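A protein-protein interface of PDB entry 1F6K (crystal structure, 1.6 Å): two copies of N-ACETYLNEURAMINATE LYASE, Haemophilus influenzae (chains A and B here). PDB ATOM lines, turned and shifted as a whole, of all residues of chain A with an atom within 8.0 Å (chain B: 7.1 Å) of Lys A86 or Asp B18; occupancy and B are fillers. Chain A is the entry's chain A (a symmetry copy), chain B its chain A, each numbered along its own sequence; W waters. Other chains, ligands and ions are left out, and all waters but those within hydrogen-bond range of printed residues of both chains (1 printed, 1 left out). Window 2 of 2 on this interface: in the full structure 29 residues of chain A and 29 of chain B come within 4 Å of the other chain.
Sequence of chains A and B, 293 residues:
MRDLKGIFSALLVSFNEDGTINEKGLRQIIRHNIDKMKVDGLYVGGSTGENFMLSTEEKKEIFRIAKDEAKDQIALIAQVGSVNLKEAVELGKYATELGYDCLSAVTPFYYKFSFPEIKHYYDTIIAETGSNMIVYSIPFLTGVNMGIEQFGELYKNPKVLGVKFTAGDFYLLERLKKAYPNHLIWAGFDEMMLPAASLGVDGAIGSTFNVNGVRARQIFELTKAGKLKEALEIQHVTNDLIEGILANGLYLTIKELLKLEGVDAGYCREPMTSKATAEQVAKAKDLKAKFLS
Among the printed residues, pairs that only touch across the chains: Val A83 with Met B53, Val A83 with Pro B271, Lys A86 with Arg B269 and Leu A85 with Pro B271.
Of the 15 printed residues of chain B, 5 touch a printed residue of chain A. Printed residues of chain A that touch a printed residue of chain B: Val A83, Asn A84, Leu A85 and Lys A86. Hydrophobic or aromatic side chains of chain A that line the printed part of chain B: Val A83 and Leu A85. Among the printed residues, no Asp or Glu carboxylate lies within 4 Å of a Lys or Arg side-chain nitrogen of the other chain.
Of the printed residues of chain B, Val A83 touches Met B53 (3.4 Å) and Pro B271 (3.4 Å). Of the printed residues of chain B, Leu A85 touches Pro B271 (3.9 Å). Lys A86 touches two residues of chain B. Phe B15 touches none of the printed residues of chain A. Of chain A, only Lys A86 comes within 4 Å of Asp B18. Of the printed residues of chain A, Met B53 touches Val A83 (3.4 Å) and Asn A84 (3.0 Å). Printed residues of chain A within 4 Å of Arg B269: Asn A84 (3.3 Å) and Lys A86 (3.5 Å). Of the printed residues of chain A, Pro B271 touches Val A83 and Leu A85. The nearest residue of chain B that does not touch Lys A86 is Gly B19 (4.04 Å).
Water W1 lies within hydrogen-bond range of OE1 of Glu B58 (2.7 Å), NH2 of Arg B269 (2.8 Å) and ND2 of Asn A84 (3.3 Å).
The backbone carbonyl oxygen (O) of Met B53 lies close to the side-chain amide oxygen (OD1) of Asn A84 (3.1 Å). The guanidinium group (NH2) of Arg B269 sits at hydrogen-bond distance from the side-chain amide oxygen (OD1) of Asn A84. The side-chain amino group of Lys A86 sits at hydrogen-bond distance from the backbone carbonyl oxygen of Asp B18 (2.9 Å). N of Ser B55 lies close to ND2 of Asn A84, at 3.4 Å.
The backbone NH (N) of Ser B55 lies within hydrogen-bond range of the side-chain carboxylate (OE1) of Glu B58, 2.9 Å away. NH2 of Arg B269 is in hydrogen-bond range of O of Met B53 (3.2 Å). OG of Ser A82 sits at hydrogen-bond distance from N of Asn A84 (3.0 Å). NH1 of Arg B269 is in salt-bridge range of OE2 of Glu B58 (2.8 Å). The backbone carbonyl oxygen of Gly B19 sits at hydrogen-bond distance from the guanidinium group of Arg B269 (2.8 Å). The side-chain amide oxygen (OD1) of Asn A84 sits at hydrogen-bond distance from the backbone NH (N) of Lys A86 (2.9 Å).
No position is printed for both chains.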
ATOM      1  N   THR A  56       6.195 -31.959 -34.363  1.00  0.00           N
ATOM      2  CA  THR A  56       7.426 -31.175 -34.250  1.00  0.00           C
ATOM      3  C   THR A  56       8.330 -31.413 -35.450  1.00  0.00           C
ATOM      4  O   THR A  56       8.890 -30.451 -36.005  1.00  0.00           O
ATOM      5  CB  THR A  56       8.174 -31.525 -32.950  1.00  0.00           C
ATOM      6  OG1 THR A  56       7.270 -31.369 -31.842  1.00  0.00           O
ATOM      7  CG2 THR A  56       9.406 -30.653 -32.782  1.00  0.00           C
ATOM      8  N   VAL A  80       7.519 -20.118 -33.308  1.00  0.00           N
ATOM      9  CA  VAL A  80       7.879 -21.390 -32.673  1.00  0.00           C
ATOM     10  C   VAL A  80       7.085 -21.668 -31.401  1.00  0.00           C
ATOM     11  O   VAL A  80       7.340 -22.649 -30.704  1.00  0.00           O
ATOM     12  CB  VAL A  80       9.385 -21.408 -32.312  1.00  0.00           C
ATOM     13  CG1 VAL A  80      10.264 -21.287 -33.567  1.00  0.00           C
ATOM     14  CG2 VAL A  80       9.771 -20.324 -31.318  1.00  0.00           C
ATOM     15  N   SER A  82       4.217 -22.635 -28.699  1.00  0.00           N
ATOM     16  CA  SER A  82       3.424 -23.860 -28.476  1.00  0.00           C
ATOM     17  C   SER A  82       2.980 -23.834 -27.016  1.00  0.00           C
ATOM     18  O   SER A  82       3.480 -23.026 -26.228  1.00  0.00           O
ATOM     19  CB  SER A  82       4.402 -25.026 -28.650  1.00  0.00           C
ATOM     20  OG  SER A  82       3.848 -26.273 -28.294  1.00  0.00           O
ATOM     21  N   VAL A  83       2.138 -24.771 -26.608  1.00  0.00           N
ATOM     22  CA  VAL A  83       1.721 -24.941 -25.212  1.00  0.00           C
ATOM     23  C   VAL A  83       2.827 -25.758 -24.549  1.00  0.00           C
ATOM     24  O   VAL A  83       3.001 -25.662 -23.330  1.00  0.00           O
ATOM     25  CB  VAL A  83       0.388 -25.714 -25.110  1.00  0.00           C
ATOM     26  CG1 VAL A  83      -0.030 -25.964 -23.643  1.00  0.00           C
ATOM     27  CG2 VAL A  83      -0.779 -25.025 -25.813  1.00  0.00           C
ATOM     28  N   ASN A  84       3.613 -26.469 -25.349  1.00  0.00           N
ATOM     29  CA  ASN A  84       4.736 -27.201 -24.784  1.00  0.00           C
ATOM     30  C   ASN A  84       5.961 -26.304 -24.920  1.00  0.00           C
ATOM     31  O   ASN A  84       6.475 -26.104 -26.018  1.00  0.00           O
ATOM     32  CB  ASN A  84       4.876 -28.523 -25.520  1.00  0.00           C
ATOM     33  CG  ASN A  84       6.082 -29.333 -25.126  1.00  0.00           C
ATOM     34  OD1 ASN A  84       6.943 -28.911 -24.352  1.00  0.00           O
ATOM     35  ND2 ASN A  84       6.199 -30.548 -25.667  1.00  0.00           N
ATOM     36  N   LEU A  85       6.439 -25.774 -23.798  1.00  0.00           N
ATOM     37  CA  LEU A  85       7.605 -24.897 -23.804  1.00  0.00           C
ATOM     38  C   LEU A  85       8.866 -25.609 -24.256  1.00  0.00           C
ATOM     39  O   LEU A  85       9.760 -25.048 -24.911  1.00  0.00           O
ATOM     40  CB  LEU A  85       7.784 -24.264 -22.419  1.00  0.00           C
ATOM     41  CG  LEU A  85       9.084 -23.470 -22.227  1.00  0.00           C
ATOM     42  CD1 LEU A  85       9.123 -22.322 -23.228  1.00  0.00           C
ATOM     43  CD2 LEU A  85       9.153 -22.928 -20.808  1.00  0.00           C
ATOM     44  N   LYS A  86       9.014 -26.900 -23.954  1.00  0.00           N
ATOM     45  CA  LYS A  86      10.192 -27.680 -24.396  1.00  0.00           C
ATOM     46  C   LYS A  86      10.203 -27.762 -25.917  1.00  0.00           C
ATOM     47  O   LYS A  86      11.279 -27.667 -26.527  1.00  0.00           O
ATOM     48  CB  LYS A  86      10.219 -29.051 -23.745  1.00  0.00           C
ATOM     49  CG  LYS A  86      10.454 -29.003 -22.231  1.00  0.00           C
ATOM     50  CD  LYS A  86      11.002 -30.375 -21.829  1.00  0.00           C
ATOM     51  CE  LYS A  86      11.207 -30.478 -20.320  1.00  0.00           C
ATOM     52  NZ  LYS A  86      12.465 -31.240 -20.043  1.00  0.00           N
ATOM     53  N   GLU A  87       9.039 -27.932 -26.531  1.00  0.00           N
ATOM     54  CA  GLU A  87       8.940 -27.971 -27.987  1.00  0.00           C
ATOM     55  C   GLU A  87       9.313 -26.596 -28.557  1.00  0.00           C
ATOM     56  O   GLU A  87      10.011 -26.496 -29.562  1.00  0.00           O
ATOM     57  CB  GLU A  87       7.536 -28.316 -28.474  1.00  0.00           C
ATOM     58  CG  GLU A  87       7.475 -28.518 -29.983  1.00  0.00           C
ATOM     59  CD  GLU A  87       6.083 -28.595 -30.551  1.00  0.00           C
ATOM     60  OE1 GLU A  87       5.135 -28.036 -29.932  1.00  0.00           O
ATOM     61  OE2 GLU A  87       5.894 -29.220 -31.612  1.00  0.00           O
ATOM     62  N   ALA A  88       8.786 -25.549 -27.915  1.00  0.00           N
ATOM     63  CA  ALA A  88       9.076 -24.192 -28.397  1.00  0.00           C
ATOM     64  C   ALA A  88      10.569 -23.913 -28.368  1.00  0.00           C
ATOM     65  O   ALA A  88      11.121 -23.295 -29.296  1.00  0.00           O
ATOM     66  CB  ALA A  88       8.318 -23.156 -27.574  1.00  0.00           C
ATOM     67  N   VAL A  89      11.256 -24.365 -27.308  1.00  0.00           N
ATOM     68  CA  VAL A  89      12.702 -24.155 -27.248  1.00  0.00           C
ATOM     69  C   VAL A  89      13.388 -24.993 -28.326  1.00  0.00           C
ATOM     70  O   VAL A  89      14.304 -24.467 -28.979  1.00  0.00           O
ATOM     71  CB  VAL A  89      13.218 -24.517 -25.852  1.00  0.00           C
ATOM     72  CG1 VAL A  89      14.730 -24.665 -25.851  1.00  0.00           C
ATOM     73  CG2 VAL A  89      12.774 -23.462 -24.840  1.00  0.00           C
ATOM     74  N   GLU A  90      12.956 -26.217 -28.544  1.00  0.00           N
ATOM     75  CA  GLU A  90      13.561 -27.071 -29.569  1.00  0.00           C
ATOM     76  C   GLU A  90      13.419 -26.434 -30.946  1.00  0.00           C
ATOM     77  O   GLU A  90      14.384 -26.382 -31.705  1.00  0.00           O
ATOM     78  CB  GLU A  90      12.918 -28.457 -29.533  1.00  0.00           C
ATOM     79  CG  GLU A  90      13.441 -29.425 -30.583  1.00  0.00           C
ATOM     80  CD  GLU A  90      12.713 -30.755 -30.609  1.00  0.00           C
ATOM     81  OE1 GLU A  90      11.861 -31.018 -29.738  1.00  0.00           O
ATOM     82  OE2 GLU A  90      12.991 -31.540 -31.539  1.00  0.00           O
ATOM     83  N   LEU A  91      12.212 -25.942 -31.250  1.00  0.00           N
ATOM     84  CA  LEU A  91      11.966 -25.310 -32.543  1.00  0.00           C
ATOM     85  C   LEU A  91      12.721 -24.005 -32.671  1.00  0.00           C
ATOM     86  O   LEU A  91      13.232 -23.672 -33.750  1.00  0.00           O
ATOM     87  CB  LEU A  91      10.455 -25.035 -32.704  1.00  0.00           C
ATOM     88  CG  LEU A  91       9.618 -26.310 -32.831  1.00  0.00           C
ATOM     89  CD1 LEU A  91       8.138 -25.994 -32.741  1.00  0.00           C
ATOM     90  CD2 LEU A  91       9.979 -27.017 -34.137  1.00  0.00           C
ATOM     91  N   GLY A  92      12.801 -23.240 -31.582  1.00  0.00           N
ATOM     92  CA  GLY A  92      13.517 -21.961 -31.639  1.00  0.00           C
ATOM     93  C   GLY A  92      14.999 -22.234 -31.888  1.00  0.00           C
ATOM     94  O   GLY A  92      15.629 -21.479 -32.637  1.00  0.00           O
ATOM     95  N   LYS A  93      15.560 -23.274 -31.257  1.00  0.00           N
ATOM     96  CA  LYS A  93      16.974 -23.579 -31.501  1.00  0.00           C
ATOM     97  C   LYS A  93      17.188 -23.970 -32.964  1.00  0.00           C
ATOM     98  O   LYS A  93      18.171 -23.508 -33.561  1.00  0.00           O
ATOM     99  CB  LYS A  93      17.474 -24.718 -30.602  1.00  0.00           C
ATOM    100  CG  LYS A  93      17.708 -24.304 -29.156  1.00  0.00           C
ATOM    101  CD  LYS A  93      18.072 -25.531 -28.316  1.00  0.00           C
ATOM    102  CE  LYS A  93      18.432 -25.207 -26.889  1.00  0.00           C
ATOM    103  NZ  LYS A  93      19.687 -24.428 -26.728  1.00  0.00           N
ATOM    104  N   TYR A 121       7.801 -17.907 -20.069  1.00  0.00           N
ATOM    105  CA  TYR A 121       7.854 -18.647 -21.342  1.00  0.00           C
ATOM    106  C   TYR A 121       8.652 -17.875 -22.386  1.00  0.00           C
ATOM    107  O   TYR A 121       9.528 -18.455 -23.031  1.00  0.00           O
ATOM    108  CB  TYR A 121       6.430 -18.873 -21.781  1.00  0.00           C
ATOM    109  CG  TYR A 121       6.013 -19.201 -23.182  1.00  0.00           C
ATOM    110  CD1 TYR A 121       5.786 -18.173 -24.096  1.00  0.00           C
ATOM    111  CD2 TYR A 121       5.792 -20.514 -23.595  1.00  0.00           C
ATOM    112  CE1 TYR A 121       5.375 -18.430 -25.394  1.00  0.00           C
ATOM    113  CE2 TYR A 121       5.353 -20.778 -24.877  1.00  0.00           C
ATOM    114  CZ  TYR A 121       5.150 -19.745 -25.770  1.00  0.00           C
ATOM    115  OH  TYR A 121       4.704 -20.069 -27.032  1.00  0.00           O
ATOM    116  N   THR A 124      12.408 -17.763 -21.409  1.00  0.00           N
ATOM    117  CA  THR A 124      13.050 -19.052 -21.573  1.00  0.00           C
ATOM    118  C   THR A 124      13.379 -19.297 -23.042  1.00  0.00           C
ATOM    119  O   THR A 124      14.504 -19.702 -23.343  1.00  0.00           O
ATOM    120  CB  THR A 124      12.173 -20.198 -21.037  1.00  0.00           C
ATOM    121  OG1 THR A 124      11.928 -20.024 -19.633  1.00  0.00           O
ATOM    122  CG2 THR A 124      12.886 -21.539 -21.210  1.00  0.00           C
ATOM    123  N   ILE A 125      12.436 -19.009 -23.941  1.00  0.00           N
ATOM    124  CA  ILE A 125      12.734 -19.212 -25.370  1.00  0.00           C
ATOM    125  C   ILE A 125      13.912 -18.348 -25.802  1.00  0.00           C
ATOM    126  O   ILE A 125      14.805 -18.841 -26.504  1.00  0.00           O
ATOM    127  CB  ILE A 125      11.527 -18.985 -26.272  1.00  0.00           C
ATOM    128  CG1 ILE A 125      10.440 -20.013 -25.918  1.00  0.00           C
ATOM    129  CG2 ILE A 125      11.897 -19.086 -27.748  1.00  0.00           C
ATOM    130  CD1 ILE A 125       9.067 -19.544 -26.392  1.00  0.00           C
ATOM    131  N   PHE B  15       6.178 -34.616 -11.949  1.00  0.00           N
ATOM    132  CA  PHE B  15       7.296 -34.222 -12.803  1.00  0.00           C
ATOM    133  C   PHE B  15       8.510 -33.937 -11.939  1.00  0.00           C
ATOM    134  O   PHE B  15       8.424 -33.504 -10.796  1.00  0.00           O
ATOM    135  CB  PHE B  15       6.994 -32.954 -13.646  1.00  0.00           C
ATOM    136  CG  PHE B  15       5.865 -33.191 -14.617  1.00  0.00           C
ATOM    137  CD1 PHE B  15       6.089 -33.791 -15.844  1.00  0.00           C
ATOM    138  CD2 PHE B  15       4.549 -32.865 -14.287  1.00  0.00           C
ATOM    139  CE1 PHE B  15       5.064 -34.052 -16.723  1.00  0.00           C
ATOM    140  CE2 PHE B  15       3.521 -33.133 -15.176  1.00  0.00           C
ATOM    141  CZ  PHE B  15       3.745 -33.722 -16.404  1.00  0.00           C
ATOM    142  N   ASN B  16       9.691 -34.130 -12.539  1.00  0.00           N
ATOM    143  CA  ASN B  16      10.935 -33.745 -11.890  1.00  0.00           C
ATOM    144  C   ASN B  16      11.104 -32.243 -12.080  1.00  0.00           C
ATOM    145  O   ASN B  16      10.377 -31.607 -12.864  1.00  0.00           O
ATOM    146  CB  ASN B  16      12.110 -34.473 -12.564  1.00  0.00           C
ATOM    147  CG  ASN B  16      12.068 -35.971 -12.271  1.00  0.00           C
ATOM    148  OD1 ASN B  16      11.922 -36.319 -11.104  1.00  0.00           O
ATOM    149  ND2 ASN B  16      12.180 -36.826 -13.266  1.00  0.00           N
ATOM    150  N   GLU B  17      12.080 -31.667 -11.395  1.00  0.00           N
ATOM    151  CA  GLU B  17      12.340 -30.233 -11.514  1.00  0.00           C
ATOM    152  C   GLU B  17      12.645 -29.804 -12.943  1.00  0.00           C
ATOM    153  O   GLU B  17      12.289 -28.687 -13.341  1.00  0.00           O
ATOM    154  CB  GLU B  17      13.504 -29.865 -10.592  1.00  0.00           C
ATOM    155  CG  GLU B  17      13.724 -28.355 -10.549  1.00  0.00           C
ATOM    156  CD  GLU B  17      14.771 -27.958  -9.535  1.00  0.00           C
ATOM    157  OE1 GLU B  17      15.456 -28.846  -8.982  1.00  0.00           O
ATOM    158  OE2 GLU B  17      14.912 -26.734  -9.311  1.00  0.00           O
ATOM    159  N   ASP B  18      13.253 -30.672 -13.743  1.00  0.00           N
ATOM    160  CA  ASP B  18      13.599 -30.335 -15.119  1.00  0.00           C
ATOM    161  C   ASP B  18      12.472 -30.589 -16.106  1.00  0.00           C
ATOM    162  O   ASP B  18      12.650 -30.413 -17.316  1.00  0.00           O
ATOM    163  CB  ASP B  18      14.873 -31.089 -15.519  1.00  0.00           C
ATOM    164  CG  ASP B  18      14.710 -32.579 -15.683  1.00  0.00           C
ATOM    165  OD1 ASP B  18      13.616 -33.143 -15.445  1.00  0.00           O
ATOM    166  OD2 ASP B  18      15.709 -33.243 -16.053  1.00  0.00           O
ATOM    167  N   GLY B  19      11.303 -31.034 -15.640  1.00  0.00           N
ATOM    168  CA  GLY B  19      10.171 -31.272 -16.498  1.00  0.00           C
ATOM    169  C   GLY B  19       9.929 -32.685 -16.962  1.00  0.00           C
ATOM    170  O   GLY B  19       8.886 -32.967 -17.558  1.00  0.00           O
ATOM    171  N   THR B  20      10.918 -33.567 -16.752  1.00  0.00           N
ATOM    172  CA  THR B  20      10.743 -34.959 -17.146  1.00  0.00           C
ATOM    173  C   THR B  20       9.781 -35.656 -16.182  1.00  0.00           C
ATOM    174  O   THR B  20       9.567 -35.184 -15.066  1.00  0.00           O
ATOM    175  CB  THR B  20      12.088 -35.705 -17.169  1.00  0.00           C
ATOM    176  OG1 THR B  20      12.730 -35.628 -15.889  1.00  0.00           O
ATOM    177  CG2 THR B  20      13.008 -35.029 -18.201  1.00  0.00           C
ATOM    178  N   ILE B  21       9.235 -36.778 -16.635  1.00  0.00           N
ATOM    179  CA  ILE B  21       8.312 -37.536 -15.782  1.00  0.00           C
ATOM    180  C   ILE B  21       9.050 -38.214 -14.637  1.00  0.00           C
ATOM    181  O   ILE B  21      10.108 -38.819 -14.845  1.00  0.00           O
ATOM    182  CB  ILE B  21       7.585 -38.591 -16.642  1.00  0.00           C
ATOM    183  CG1 ILE B  21       6.708 -37.890 -17.676  1.00  0.00           C
ATOM    184  CG2 ILE B  21       6.750 -39.520 -15.772  1.00  0.00           C
ATOM    185  CD1 ILE B  21       6.509 -38.684 -18.955  1.00  0.00           C
ATOM    186  N   MET B  53       0.973 -29.770 -22.466  1.00  0.00           N
ATOM    187  CA  MET B  53       2.303 -29.202 -22.438  1.00  0.00           C
ATOM    188  C   MET B  53       3.366 -30.259 -22.741  1.00  0.00           C
ATOM    189  O   MET B  53       4.560 -29.937 -22.629  1.00  0.00           O
ATOM    190  CB  MET B  53       2.576 -28.632 -21.045  1.00  0.00           C
ATOM    191  CG  MET B  53       1.740 -27.414 -20.693  1.00  0.00           C
ATOM    192  SD  MET B  53       2.064 -26.774 -19.042  1.00  0.00           S
ATOM    193  CE  MET B  53       1.439 -28.104 -18.022  1.00  0.00           C
ATOM    194  N   SER B  55       5.269 -33.735 -24.904  1.00  0.00           N
ATOM    195  CA  SER B  55       5.497 -34.286 -26.241  1.00  0.00           C
ATOM    196  C   SER B  55       4.686 -35.563 -26.409  1.00  0.00           C
ATOM    197  O   SER B  55       4.216 -36.181 -25.451  1.00  0.00           O
ATOM    198  CB  SER B  55       6.982 -34.637 -26.455  1.00  0.00           C
ATOM    199  OG  SER B  55       7.324 -35.747 -25.615  1.00  0.00           O
ATOM    200  N   GLU B  58       6.273 -38.337 -24.400  1.00  0.00           N
ATOM    201  CA  GLU B  58       5.973 -38.207 -22.964  1.00  0.00           C
ATOM    202  C   GLU B  58       4.564 -38.690 -22.666  1.00  0.00           C
ATOM    203  O   GLU B  58       4.326 -39.398 -21.675  1.00  0.00           O
ATOM    204  CB  GLU B  58       6.141 -36.749 -22.505  1.00  0.00           C
ATOM    205  CG  GLU B  58       7.618 -36.370 -22.430  1.00  0.00           C
ATOM    206  CD  GLU B  58       7.864 -34.896 -22.185  1.00  0.00           C
ATOM    207  OE1 GLU B  58       7.086 -34.070 -22.702  1.00  0.00           O
ATOM    208  OE2 GLU B  58       8.848 -34.572 -21.491  1.00  0.00           O
ATOM    209  N   TYR B 267       6.861 -31.817  -9.071  1.00  0.00           N
ATOM    210  CA  TYR B 267       6.658 -30.474  -9.589  1.00  0.00           C
ATOM    211  C   TYR B 267       5.595 -30.441 -10.690  1.00  0.00           C
ATOM    212  O   TYR B 267       5.118 -31.457 -11.183  1.00  0.00           O
ATOM    213  CB  TYR B 267       7.974 -30.036 -10.275  1.00  0.00           C
ATOM    214  CG  TYR B 267       9.153 -29.913  -9.339  1.00  0.00           C
ATOM    215  CD1 TYR B 267       9.852 -31.017  -8.865  1.00  0.00           C
ATOM    216  CD2 TYR B 267       9.572 -28.645  -8.958  1.00  0.00           C
ATOM    217  CE1 TYR B 267      10.917 -30.848  -7.997  1.00  0.00           C
ATOM    218  CE2 TYR B 267      10.632 -28.477  -8.090  1.00  0.00           C
ATOM    219  CZ  TYR B 267      11.302 -29.584  -7.624  1.00  0.00           C
ATOM    220  OH  TYR B 267      12.369 -29.406  -6.760  1.00  0.00           O
ATOM    221  N   CYS B 268       5.219 -29.200 -11.045  1.00  0.00           N
ATOM    222  CA  CYS B 268       4.316 -29.013 -12.188  1.00  0.00           C
ATOM    223  C   CYS B 268       5.239 -28.776 -13.394  1.00  0.00           C
ATOM    224  O   CYS B 268       6.411 -28.432 -13.201  1.00  0.00           O
ATOM    225  CB  CYS B 268       3.349 -27.857 -12.034  1.00  0.00           C
ATOM    226  SG  CYS B 268       1.866 -28.231 -11.079  1.00  0.00           S
ATOM    227  N   ARG B 269       4.688 -28.965 -14.584  1.00  0.00           N
ATOM    228  CA  ARG B 269       5.492 -28.819 -15.811  1.00  0.00           C
ATOM    229  C   ARG B 269       5.454 -27.415 -16.401  1.00  0.00           C
ATOM    230  O   ARG B 269       4.365 -26.872 -16.607  1.00  0.00           O
ATOM    231  CB  ARG B 269       4.881 -29.811 -16.802  1.00  0.00           C
ATOM    232  CG  ARG B 269       5.328 -29.700 -18.247  1.00  0.00           C
ATOM    233  CD  ARG B 269       6.761 -30.171 -18.467  1.00  0.00           C
ATOM    234  NE  ARG B 269       6.978 -30.176 -19.919  1.00  0.00           N
ATOM    235  CZ  ARG B 269       7.484 -31.182 -20.623  1.00  0.00           C
ATOM    236  NH1 ARG B 269       7.873 -32.317 -20.064  1.00  0.00           N
ATOM    237  NH2 ARG B 269       7.540 -31.016 -21.943  1.00  0.00           N
ATOM    238  N   GLU B 270       6.617 -26.852 -16.730  1.00  0.00           N
ATOM    239  CA  GLU B 270       6.646 -25.548 -17.389  1.00  0.00           C
ATOM    240  C   GLU B 270       6.076 -25.465 -18.787  1.00  0.00           C
ATOM    241  O   GLU B 270       6.155 -26.612 -19.181  1.00  0.00           O
ATOM    242  CB  GLU B 270       8.105 -25.032 -17.436  1.00  0.00           C
ATOM    243  CG  GLU B 270       8.630 -24.671 -16.057  1.00  0.00           C
ATOM    244  CD  GLU B 270       9.960 -23.962 -16.037  1.00  0.00           C
ATOM    245  OE1 GLU B 270      10.516 -23.609 -17.100  1.00  0.00           O
ATOM    246  OE2 GLU B 270      10.457 -23.763 -14.901  1.00  0.00           O
ATOM    247  N   PRO B 271       5.097 -24.618 -19.025  1.00  0.00           N
ATOM    248  CA  PRO B 271       5.043 -23.212 -18.754  1.00  0.00           C
ATOM    249  C   PRO B 271       4.220 -22.970 -17.483  1.00  0.00           C
ATOM    250  O   PRO B 271       4.136 -21.827 -17.013  1.00  0.00           O
ATOM    251  CB  PRO B 271       4.575 -22.430 -19.960  1.00  0.00           C
ATOM    252  CG  PRO B 271       3.763 -23.430 -20.693  1.00  0.00           C
ATOM    253  CD  PRO B 271       4.503 -24.678 -20.388  1.00  0.00           C
HETATM  254  O   HOH W   1       8.572 -32.352 -24.160  1.00  0.00           O
